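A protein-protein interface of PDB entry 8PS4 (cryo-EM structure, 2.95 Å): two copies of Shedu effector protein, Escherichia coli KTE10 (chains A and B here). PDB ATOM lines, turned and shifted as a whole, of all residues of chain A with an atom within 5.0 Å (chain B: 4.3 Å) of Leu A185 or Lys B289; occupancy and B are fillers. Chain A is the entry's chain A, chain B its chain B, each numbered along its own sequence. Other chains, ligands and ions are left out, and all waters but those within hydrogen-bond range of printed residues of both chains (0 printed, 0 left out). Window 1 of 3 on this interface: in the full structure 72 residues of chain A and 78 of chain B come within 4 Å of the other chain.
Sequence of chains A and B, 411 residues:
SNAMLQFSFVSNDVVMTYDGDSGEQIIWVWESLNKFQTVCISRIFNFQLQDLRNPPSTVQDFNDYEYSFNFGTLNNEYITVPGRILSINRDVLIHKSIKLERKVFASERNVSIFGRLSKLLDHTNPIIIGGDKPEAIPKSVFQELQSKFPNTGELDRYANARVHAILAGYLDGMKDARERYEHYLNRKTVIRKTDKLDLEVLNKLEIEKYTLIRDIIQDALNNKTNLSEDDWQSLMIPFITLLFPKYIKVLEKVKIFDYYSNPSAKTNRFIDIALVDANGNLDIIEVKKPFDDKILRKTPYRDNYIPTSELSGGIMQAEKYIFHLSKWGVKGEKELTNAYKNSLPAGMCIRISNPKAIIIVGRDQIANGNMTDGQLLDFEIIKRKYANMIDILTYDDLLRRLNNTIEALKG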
ATOM      1  N   GLU A 154     -30.125 -35.577 -10.132  1.00  0.00           N
ATOM      2  CA  GLU A 154     -28.925 -35.053 -10.840  1.00  0.00           C
ATOM      3  C   GLU A 154     -28.750 -35.916 -12.090  1.00  0.00           C
ATOM      4  O   GLU A 154     -28.479 -35.356 -13.171  1.00  0.00           O
ATOM      5  CB  GLU A 154     -27.697 -35.103  -9.928  1.00  0.00           C
ATOM      6  CG  GLU A 154     -26.542 -34.239 -10.405  1.00  0.00           C
ATOM      7  CD  GLU A 154     -25.668 -34.858 -11.483  1.00  0.00           C
ATOM      8  OE1 GLU A 154     -25.487 -36.091 -11.462  1.00  0.00           O
ATOM      9  OE2 GLU A 154     -25.183 -34.106 -12.349  1.00  0.00           O
ATOM     10  N   ARG A 178     -30.573 -29.133 -21.117  1.00  0.00           N
ATOM     11  CA  ARG A 178     -29.092 -29.019 -21.072  1.00  0.00           C
ATOM     12  C   ARG A 178     -28.697 -27.797 -20.237  1.00  0.00           C
ATOM     13  O   ARG A 178     -27.790 -27.931 -19.399  1.00  0.00           O
ATOM     14  CB  ARG A 178     -28.500 -28.946 -22.482  1.00  0.00           C
ATOM     15  CG  ARG A 178     -27.037 -28.530 -22.498  1.00  0.00           C
ATOM     16  CD  ARG A 178     -26.255 -29.027 -23.694  1.00  0.00           C
ATOM     17  NE  ARG A 178     -24.884 -28.547 -23.608  1.00  0.00           N
ATOM     18  CZ  ARG A 178     -23.938 -28.814 -24.496  1.00  0.00           C
ATOM     19  NH1 ARG A 178     -24.211 -29.568 -25.547  1.00  0.00           N
ATOM     20  NH2 ARG A 178     -22.721 -28.331 -24.325  1.00  0.00           N
ATOM     21  N   TYR A 181     -29.122 -28.576 -16.557  1.00  0.00           N
ATOM     22  CA  TYR A 181     -28.128 -29.570 -16.076  1.00  0.00           C
ATOM     23  C   TYR A 181     -26.765 -28.891 -15.914  1.00  0.00           C
ATOM     24  O   TYR A 181     -26.107 -29.103 -14.876  1.00  0.00           O
ATOM     25  CB  TYR A 181     -28.052 -30.755 -17.042  1.00  0.00           C
ATOM     26  CG  TYR A 181     -26.815 -31.608 -16.913  1.00  0.00           C
ATOM     27  CD1 TYR A 181     -26.563 -32.337 -15.763  1.00  0.00           C
ATOM     28  CD2 TYR A 181     -25.899 -31.695 -17.949  1.00  0.00           C
ATOM     29  CE1 TYR A 181     -25.428 -33.122 -15.640  1.00  0.00           C
ATOM     30  CE2 TYR A 181     -24.761 -32.477 -17.843  1.00  0.00           C
ATOM     31  CZ  TYR A 181     -24.525 -33.195 -16.685  1.00  0.00           C
ATOM     32  OH  TYR A 181     -23.406 -33.968 -16.575  1.00  0.00           O
ATOM     33  N   GLU A 182     -26.377 -28.074 -16.896  1.00  0.00           N
ATOM     34  CA  GLU A 182     -25.056 -27.397 -16.840  1.00  0.00           C
ATOM     35  C   GLU A 182     -25.030 -26.440 -15.645  1.00  0.00           C
ATOM     36  O   GLU A 182     -24.000 -26.396 -14.962  1.00  0.00           O
ATOM     37  CB  GLU A 182     -24.730 -26.693 -18.159  1.00  0.00           C
ATOM     38  CG  GLU A 182     -24.585 -27.644 -19.336  1.00  0.00           C
ATOM     39  CD  GLU A 182     -23.454 -28.657 -19.256  1.00  0.00           C
ATOM     40  OE1 GLU A 182     -22.496 -28.424 -18.493  1.00  0.00           O
ATOM     41  OE2 GLU A 182     -23.535 -29.680 -19.964  1.00  0.00           O
ATOM     42  N   HIS A 183     -26.128 -25.716 -15.404  1.00  0.00           N
ATOM     43  CA  HIS A 183     -26.168 -24.731 -14.291  1.00  0.00           C
ATOM     44  C   HIS A 183     -25.991 -25.449 -12.948  1.00  0.00           C
ATOM     45  O   HIS A 183     -25.194 -24.962 -12.121  1.00  0.00           O
ATOM     46  CB  HIS A 183     -27.473 -23.925 -14.340  1.00  0.00           C
ATOM     47  CG  HIS A 183     -27.876 -23.353 -13.022  1.00  0.00           C
ATOM     48  ND1 HIS A 183     -28.840 -23.941 -12.226  1.00  0.00           N
ATOM     49  CD2 HIS A 183     -27.445 -22.262 -12.352  1.00  0.00           C
ATOM     50  CE1 HIS A 183     -28.989 -23.236 -11.124  1.00  0.00           C
ATOM     51  NE2 HIS A 183     -28.145 -22.199 -11.178  1.00  0.00           N
ATOM     52  N   TYR A 184     -26.686 -26.575 -12.756  1.00  0.00           N
ATOM     53  CA  TYR A 184     -26.571 -27.345 -11.489  1.00  0.00           C
ATOM     54  C   TYR A 184     -25.140 -27.875 -11.352  1.00  0.00           C
ATOM     55  O   TYR A 184     -24.584 -27.819 -10.238  1.00  0.00           O
ATOM     56  CB  TYR A 184     -27.617 -28.461 -11.438  1.00  0.00           C
ATOM     57  CG  TYR A 184     -28.977 -28.027 -10.951  1.00  0.00           C
ATOM     58  CD1 TYR A 184     -29.781 -27.196 -11.713  1.00  0.00           C
ATOM     59  CD2 TYR A 184     -29.467 -28.450  -9.727  1.00  0.00           C
ATOM     60  CE1 TYR A 184     -31.030 -26.794 -11.273  1.00  0.00           C
ATOM     61  CE2 TYR A 184     -30.714 -28.059  -9.272  1.00  0.00           C
ATOM     62  CZ  TYR A 184     -31.501 -27.228 -10.049  1.00  0.00           C
ATOM     63  OH  TYR A 184     -32.732 -26.836  -9.609  1.00  0.00           O
ATOM     64  N   LEU A 185     -24.568 -28.367 -12.454  1.00  0.00           N
ATOM     65  CA  LEU A 185     -23.167 -28.866 -12.441  1.00  0.00           C
ATOM     66  C   LEU A 185     -22.217 -27.701 -12.144  1.00  0.00           C
ATOM     67  O   LEU A 185     -21.253 -27.921 -11.395  1.00  0.00           O
ATOM     68  CB  LEU A 185     -22.854 -29.506 -13.796  1.00  0.00           C
ATOM     69  CG  LEU A 185     -21.972 -30.752 -13.742  1.00  0.00           C
ATOM     70  CD1 LEU A 185     -22.624 -31.835 -12.897  1.00  0.00           C
ATOM     71  CD2 LEU A 185     -21.683 -31.273 -15.140  1.00  0.00           C
ATOM     72  N   ASN A 186     -22.494 -26.511 -12.689  1.00  0.00           N
ATOM     73  CA  ASN A 186     -21.587 -25.339 -12.528  1.00  0.00           C
ATOM     74  C   ASN A 186     -21.448 -24.969 -11.048  1.00  0.00           C
ATOM     75  O   ASN A 186     -20.338 -24.567 -10.647  1.00  0.00           O
ATOM     76  CB  ASN A 186     -22.026 -24.143 -13.375  1.00  0.00           C
ATOM     77  CG  ASN A 186     -21.667 -24.299 -14.837  1.00  0.00           C
ATOM     78  OD1 ASN A 186     -21.091 -25.309 -15.232  1.00  0.00           O
ATOM     79  ND2 ASN A 186     -22.004 -23.308 -15.646  1.00  0.00           N
ATOM     80  N   ARG A 187     -22.532 -25.089 -10.277  1.00  0.00           N
ATOM     81  CA  ARG A 187     -22.476 -24.763  -8.829  1.00  0.00           C
ATOM     82  C   ARG A 187     -21.443 -25.682  -8.168  1.00  0.00           C
ATOM     83  O   ARG A 187     -20.669 -25.184  -7.329  1.00  0.00           O
ATOM     84  CB  ARG A 187     -23.850 -24.957  -8.183  1.00  0.00           C
ATOM     85  CG  ARG A 187     -24.990 -24.258  -8.911  1.00  0.00           C
ATOM     86  CD  ARG A 187     -26.320 -24.685  -8.328  1.00  0.00           C
ATOM     87  NE  ARG A 187     -26.314 -26.113  -8.046  1.00  0.00           N
ATOM     88  CZ  ARG A 187     -27.313 -26.773  -7.474  1.00  0.00           C
ATOM     89  NH1 ARG A 187     -28.414 -26.133  -7.121  1.00  0.00           N
ATOM     90  NH2 ARG A 187     -27.206 -28.072  -7.258  1.00  0.00           N
ATOM     91  N   LYS A 188     -21.428 -26.968  -8.536  1.00  0.00           N
ATOM     92  CA  LYS A 188     -20.390 -27.896  -8.009  1.00  0.00           C
ATOM     93  C   LYS A 188     -19.034 -27.511  -8.610  1.00  0.00           C
ATOM     94  O   LYS A 188     -18.990 -27.195  -9.814  1.00  0.00           O
ATOM     95  CB  LYS A 188     -20.736 -29.342  -8.370  1.00  0.00           C
ATOM     96  CG  LYS A 188     -22.121 -29.810  -7.947  1.00  0.00           C
ATOM     97  CD  LYS A 188     -22.461 -31.196  -8.452  1.00  0.00           C
ATOM     98  CE  LYS A 188     -23.799 -31.698  -7.953  1.00  0.00           C
ATOM     99  NZ  LYS A 188     -23.820 -31.822  -6.476  1.00  0.00           N
ATOM    100  N   THR A 189     -17.971 -27.531  -7.797  1.00  0.00           N
ATOM    101  CA  THR A 189     -16.599 -27.225  -8.291  1.00  0.00           C
ATOM    102  C   THR A 189     -15.682 -28.405  -7.957  1.00  0.00           C
ATOM    103  O   THR A 189     -15.098 -28.402  -6.855  1.00  0.00           O
ATOM    104  CB  THR A 189     -16.079 -25.903  -7.712  1.00  0.00           C
ATOM    105  OG1 THR A 189     -16.339 -25.902  -6.308  1.00  0.00           O
ATOM    106  CG2 THR A 189     -16.720 -24.688  -8.345  1.00  0.00           C
ATOM    107  N   TYR B 158     -22.193 -43.074 -16.083  1.00  0.00           N
ATOM    108  CA  TYR B 158     -22.018 -41.624 -15.807  1.00  0.00           C
ATOM    109  C   TYR B 158     -21.750 -41.419 -14.313  1.00  0.00           C
ATOM    110  O   TYR B 158     -20.865 -40.617 -13.970  1.00  0.00           O
ATOM    111  CB  TYR B 158     -23.247 -40.826 -16.248  1.00  0.00           C
ATOM    112  CG  TYR B 158     -23.301 -39.424 -15.693  1.00  0.00           C
ATOM    113  CD1 TYR B 158     -22.419 -38.449 -16.126  1.00  0.00           C
ATOM    114  CD2 TYR B 158     -24.228 -39.074 -14.724  1.00  0.00           C
ATOM    115  CE1 TYR B 158     -22.455 -37.163 -15.614  1.00  0.00           C
ATOM    116  CE2 TYR B 158     -24.278 -37.793 -14.202  1.00  0.00           C
ATOM    117  CZ  TYR B 158     -23.390 -36.832 -14.650  1.00  0.00           C
ATOM    118  OH  TYR B 158     -23.433 -35.567 -14.142  1.00  0.00           O
ATOM    119  N   ARG B 162     -18.586 -39.652 -12.805  1.00  0.00           N
ATOM    120  CA  ARG B 162     -18.722 -38.409 -11.997  1.00  0.00           C
ATOM    121  C   ARG B 162     -18.083 -38.604 -10.617  1.00  0.00           C
ATOM    122  O   ARG B 162     -17.324 -37.714 -10.197  1.00  0.00           O
ATOM    123  CB  ARG B 162     -20.200 -38.019 -11.883  1.00  0.00           C
ATOM    124  CG  ARG B 162     -20.449 -36.693 -11.177  1.00  0.00           C
ATOM    125  CD  ARG B 162     -19.771 -35.522 -11.861  1.00  0.00           C
ATOM    126  NE  ARG B 162     -19.987 -34.278 -11.138  1.00  0.00           N
ATOM    127  CZ  ARG B 162     -19.462 -33.107 -11.482  1.00  0.00           C
ATOM    128  NH1 ARG B 162     -18.681 -33.017 -12.544  1.00  0.00           N
ATOM    129  NH2 ARG B 162     -19.717 -32.030 -10.760  1.00  0.00           N
ATOM    130  N   THR B 225     -14.149 -34.653 -19.256  1.00  0.00           N
ATOM    131  CA  THR B 225     -15.390 -34.193 -19.937  1.00  0.00           C
ATOM    132  C   THR B 225     -16.536 -34.025 -18.931  1.00  0.00           C
ATOM    133  O   THR B 225     -17.291 -33.048 -19.078  1.00  0.00           O
ATOM    134  CB  THR B 225     -15.771 -35.136 -21.084  1.00  0.00           C
ATOM    135  OG1 THR B 225     -16.834 -34.526 -21.818  1.00  0.00           O
ATOM    136  CG2 THR B 225     -16.201 -36.503 -20.599  1.00  0.00           C
ATOM    137  N   ASN B 226     -16.667 -34.932 -17.957  1.00  0.00           N
ATOM    138  CA  ASN B 226     -17.809 -34.890 -16.999  1.00  0.00           C
ATOM    139  C   ASN B 226     -17.723 -33.660 -16.087  1.00  0.00           C
ATOM    140  O   ASN B 226     -18.696 -33.421 -15.350  1.00  0.00           O
ATOM    141  CB  ASN B 226     -17.891 -36.172 -16.167  1.00  0.00           C
ATOM    142  CG  ASN B 226     -17.628 -37.420 -16.980  1.00  0.00           C
ATOM    143  OD1 ASN B 226     -16.481 -37.835 -17.136  1.00  0.00           O
ATOM    144  ND2 ASN B 226     -18.682 -38.026 -17.502  1.00  0.00           N
ATOM    145  N   LEU B 227     -16.618 -32.910 -16.138  1.00  0.00           N
ATOM    146  CA  LEU B 227     -16.420 -31.728 -15.259  1.00  0.00           C
ATOM    147  C   LEU B 227     -17.423 -30.634 -15.636  1.00  0.00           C
ATOM    148  O   LEU B 227     -17.907 -30.649 -16.778  1.00  0.00           O
ATOM    149  CB  LEU B 227     -14.979 -31.227 -15.394  1.00  0.00           C
ATOM    150  CG  LEU B 227     -14.062 -31.530 -14.210  1.00  0.00           C
ATOM    151  CD1 LEU B 227     -14.007 -33.023 -13.933  1.00  0.00           C
ATOM    152  CD2 LEU B 227     -12.666 -30.988 -14.464  1.00  0.00           C
ATOM    153  N   SER B 228     -17.704 -29.717 -14.708  1.00  0.00           N
ATOM    154  CA  SER B 228     -18.678 -28.623 -14.958  1.00  0.00           C
ATOM    155  C   SER B 228     -18.127 -27.664 -16.015  1.00  0.00           C
ATOM    156  O   SER B 228     -16.899 -27.636 -16.201  1.00  0.00           O
ATOM    157  CB  SER B 228     -18.974 -27.892 -13.683  1.00  0.00           C
ATOM    158  OG  SER B 228     -17.809 -27.247 -13.189  1.00  0.00           O
ATOM    159  N   VAL B 287     -15.230 -21.046 -24.573  1.00  0.00           N
ATOM    160  CA  VAL B 287     -14.760 -22.454 -24.417  1.00  0.00           C
ATOM    161  C   VAL B 287     -15.961 -23.244 -23.897  1.00  0.00           C
ATOM    162  O   VAL B 287     -16.361 -23.005 -22.742  1.00  0.00           O
ATOM    163  CB  VAL B 287     -13.543 -22.534 -23.475  1.00  0.00           C
ATOM    164  CG1 VAL B 287     -13.155 -23.967 -23.157  1.00  0.00           C
ATOM    165  CG2 VAL B 287     -12.352 -21.778 -24.039  1.00  0.00           C
ATOM    166  N   LYS B 288     -16.533 -24.126 -24.721  1.00  0.00           N
ATOM    167  CA  LYS B 288     -17.787 -24.815 -24.318  1.00  0.00           C
ATOM    168  C   LYS B 288     -17.526 -26.305 -24.093  1.00  0.00           C
ATOM    169  O   LYS B 288     -16.915 -26.932 -24.974  1.00  0.00           O
ATOM    170  CB  LYS B 288     -18.867 -24.601 -25.383  1.00  0.00           C
ATOM    171  CG  LYS B 288     -19.264 -23.152 -25.628  1.00  0.00           C
ATOM    172  CD  LYS B 288     -19.903 -22.497 -24.424  1.00  0.00           C
ATOM    173  CE  LYS B 288     -20.362 -21.079 -24.694  1.00  0.00           C
ATOM    174  NZ  LYS B 288     -20.962 -20.456 -23.489  1.00  0.00           N
ATOM    175  N   LYS B 289     -17.990 -26.841 -22.962  1.00  0.00           N
ATOM    176  CA  LYS B 289     -17.835 -28.291 -22.673  1.00  0.00           C
ATOM    177  C   LYS B 289     -18.341 -29.100 -23.882  1.00  0.00           C
ATOM    178  O   LYS B 289     -19.478 -28.816 -24.309  1.00  0.00           O
ATOM    179  CB  LYS B 289     -18.617 -28.644 -21.406  1.00  0.00           C
ATOM    180  CG  LYS B 289     -18.359 -30.024 -20.821  1.00  0.00           C
ATOM    181  CD  LYS B 289     -19.258 -30.320 -19.643  1.00  0.00           C
ATOM    182  CE  LYS B 289     -20.345 -31.324 -19.960  1.00  0.00           C
ATOM    183  NZ  LYS B 289     -21.236 -31.550 -18.798  1.00  0.00           N
ATOM    184  N   PRO B 290     -17.601 -30.079 -24.471  1.00  0.00           N
ATOM    185  CA  PRO B 290     -18.144 -30.827 -25.606  1.00  0.00           C
ATOM    186  C   PRO B 290     -19.125 -31.918 -25.152  1.00  0.00           C
ATOM    187  O   PRO B 290     -18.838 -33.086 -25.350  1.00  0.00           O
ATOM    188  CB  PRO B 290     -16.888 -31.458 -26.224  1.00  0.00           C
ATOM    189  CG  PRO B 290     -15.937 -31.638 -25.057  1.00  0.00           C
ATOM    190  CD  PRO B 290     -16.258 -30.519 -24.088  1.00  0.00           C
ATOM    191  N   PHE B 291     -20.263 -31.518 -24.582  1.00  0.00           N
ATOM    192  CA  PHE B 291     -21.296 -32.507 -24.183  1.00  0.00           C
ATOM    193  C   PHE B 291     -21.780 -33.244 -25.436  1.00  0.00           C
ATOM    194  O   PHE B 291     -21.814 -34.489 -25.422  1.00  0.00           O
ATOM    195  CB  PHE B 291     -22.441 -31.800 -23.454  1.00  0.00           C
ATOM    196  CG  PHE B 291     -23.462 -32.710 -22.823  1.00  0.00           C
ATOM    197  CD1 PHE B 291     -23.216 -33.313 -21.602  1.00  0.00           C
ATOM    198  CD2 PHE B 291     -24.675 -32.954 -23.446  1.00  0.00           C
ATOM    199  CE1 PHE B 291     -24.157 -34.146 -21.019  1.00  0.00           C
ATOM    200  CE2 PHE B 291     -25.614 -33.789 -22.863  1.00  0.00           C
ATOM    201  CZ  PHE B 291     -25.354 -34.383 -21.651  1.00  0.00           C
ATOM    202  N   GLU B 310     -26.163 -26.471 -30.528  1.00  0.00           N
ATOM    203  CA  GLU B 310     -25.038 -26.115 -29.626  1.00  0.00           C
ATOM    204  C   GLU B 310     -24.110 -25.116 -30.324  1.00  0.00           C
ATOM    205  O   GLU B 310     -23.743 -24.113 -29.685  1.00  0.00           O
ATOM    206  CB  GLU B 310     -24.268 -27.385 -29.262  1.00  0.00           C
ATOM    207  CG  GLU B 310     -23.279 -27.210 -28.128  1.00  0.00           C
ATOM    208  CD  GLU B 310     -22.200 -28.280 -28.087  1.00  0.00           C
ATOM    209  OE1 GLU B 310     -22.009 -28.960 -29.115  1.00  0.00           O
ATOM    210  OE2 GLU B 310     -21.551 -28.428 -27.033  1.00  0.00           O
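The side-chain amino group (NZ) of Lys B289 lies within salt-bridge range of the side-chain carboxylate (OE2) of Glu A182 (3.2 Å). The guanidinium group of Arg A178 lies within salt-bridge range of the side-chain carboxylate of Glu B310. The side-chain carboxylate (OE2) of Glu A154 lies within hydrogen-bond range of the side-chain hydroxyl (OH) of Tyr B158 (2.9 Å). The backbone carbonyl oxygen (O) of Lys B289 is in hydrogen-bond range of the guanidinium group (NH2) of Arg A178, at 3.3 Å. The side-chain hydroxyl of Tyr B158 lies within hydrogen-bond range of the side-chain hydroxyl of Tyr A181 (2.9 Å).
The side-chain amide oxygen (OD1) of Asn A186 lies close to the backbone carbonyl oxygen (O) of Glu A182 (3.1 Å). O of Asn B226 sits at hydrogen-bond distance from NH1 of Arg B162, 2.8 Å away.
Among the printed residues, pairs that only touch across the chains: Leu A185 with Ser B228 (3.2 Å), Arg A178 with Phe B291 (3.5 Å), Lys A188 with Ser B228 (3.6 Å), Leu A185 with Arg B162 (3.6 Å), Tyr A181 with Phe B291 (3.6 Å), Lys A188 with Arg B162 (3.7 Å), Asn A186 with Ser B228 (3.7 Å), Leu A185 with Asn B226 (3.7 Å), Leu A185 with Lys B289 (3.7 Å), Tyr A181 with Lys B289 (3.8 Å) and Glu A182 with Phe B291 (3.998 Å).
Printed residues of chain B within 4 Å of Leu A185: Arg B162, Asn B226, Ser B228 and Lys B289. Lys B289 touches just these residues of chain A: Arg A178, Tyr A181, Glu A182 and Leu A185. Of the printed residues of chain B, Lys A188 touches Arg B162 and Ser B228. Of the printed residues of chain A, Glu B310 touches Arg A178 (3.0 Å). The nearest printed residue of chain A that does not touch Lys B289 is Asn A186 (6.9 Å). The nearest printed residue of chain A that does not touch Ser B228 is Thr A189 (5.0 Å).
Hydrophobic or aromatic side chains of chain A that line the printed part of chain B: Tyr A181 and Leu A185. Printed residues of chain B that touch a printed residue of chain A: Tyr B158, Arg B162, Asn B226, Ser B228, Lys B289, Phe B291 and Glu B310. Among the printed residues, 16 pairs touch across the chains. Among the printed residues, Asp or Glu carboxylates within 4 Å of a Lys or Arg side-chain nitrogen of the other chain: Arg A178 with Glu B310 (3.0 Å) and Glu A182 with Lys B289 (3.2 Å).
No position is printed for both chains. Of the 16 pairs that touch across the chains among the printed residues, none has its exchanged pair printed and touching as well.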
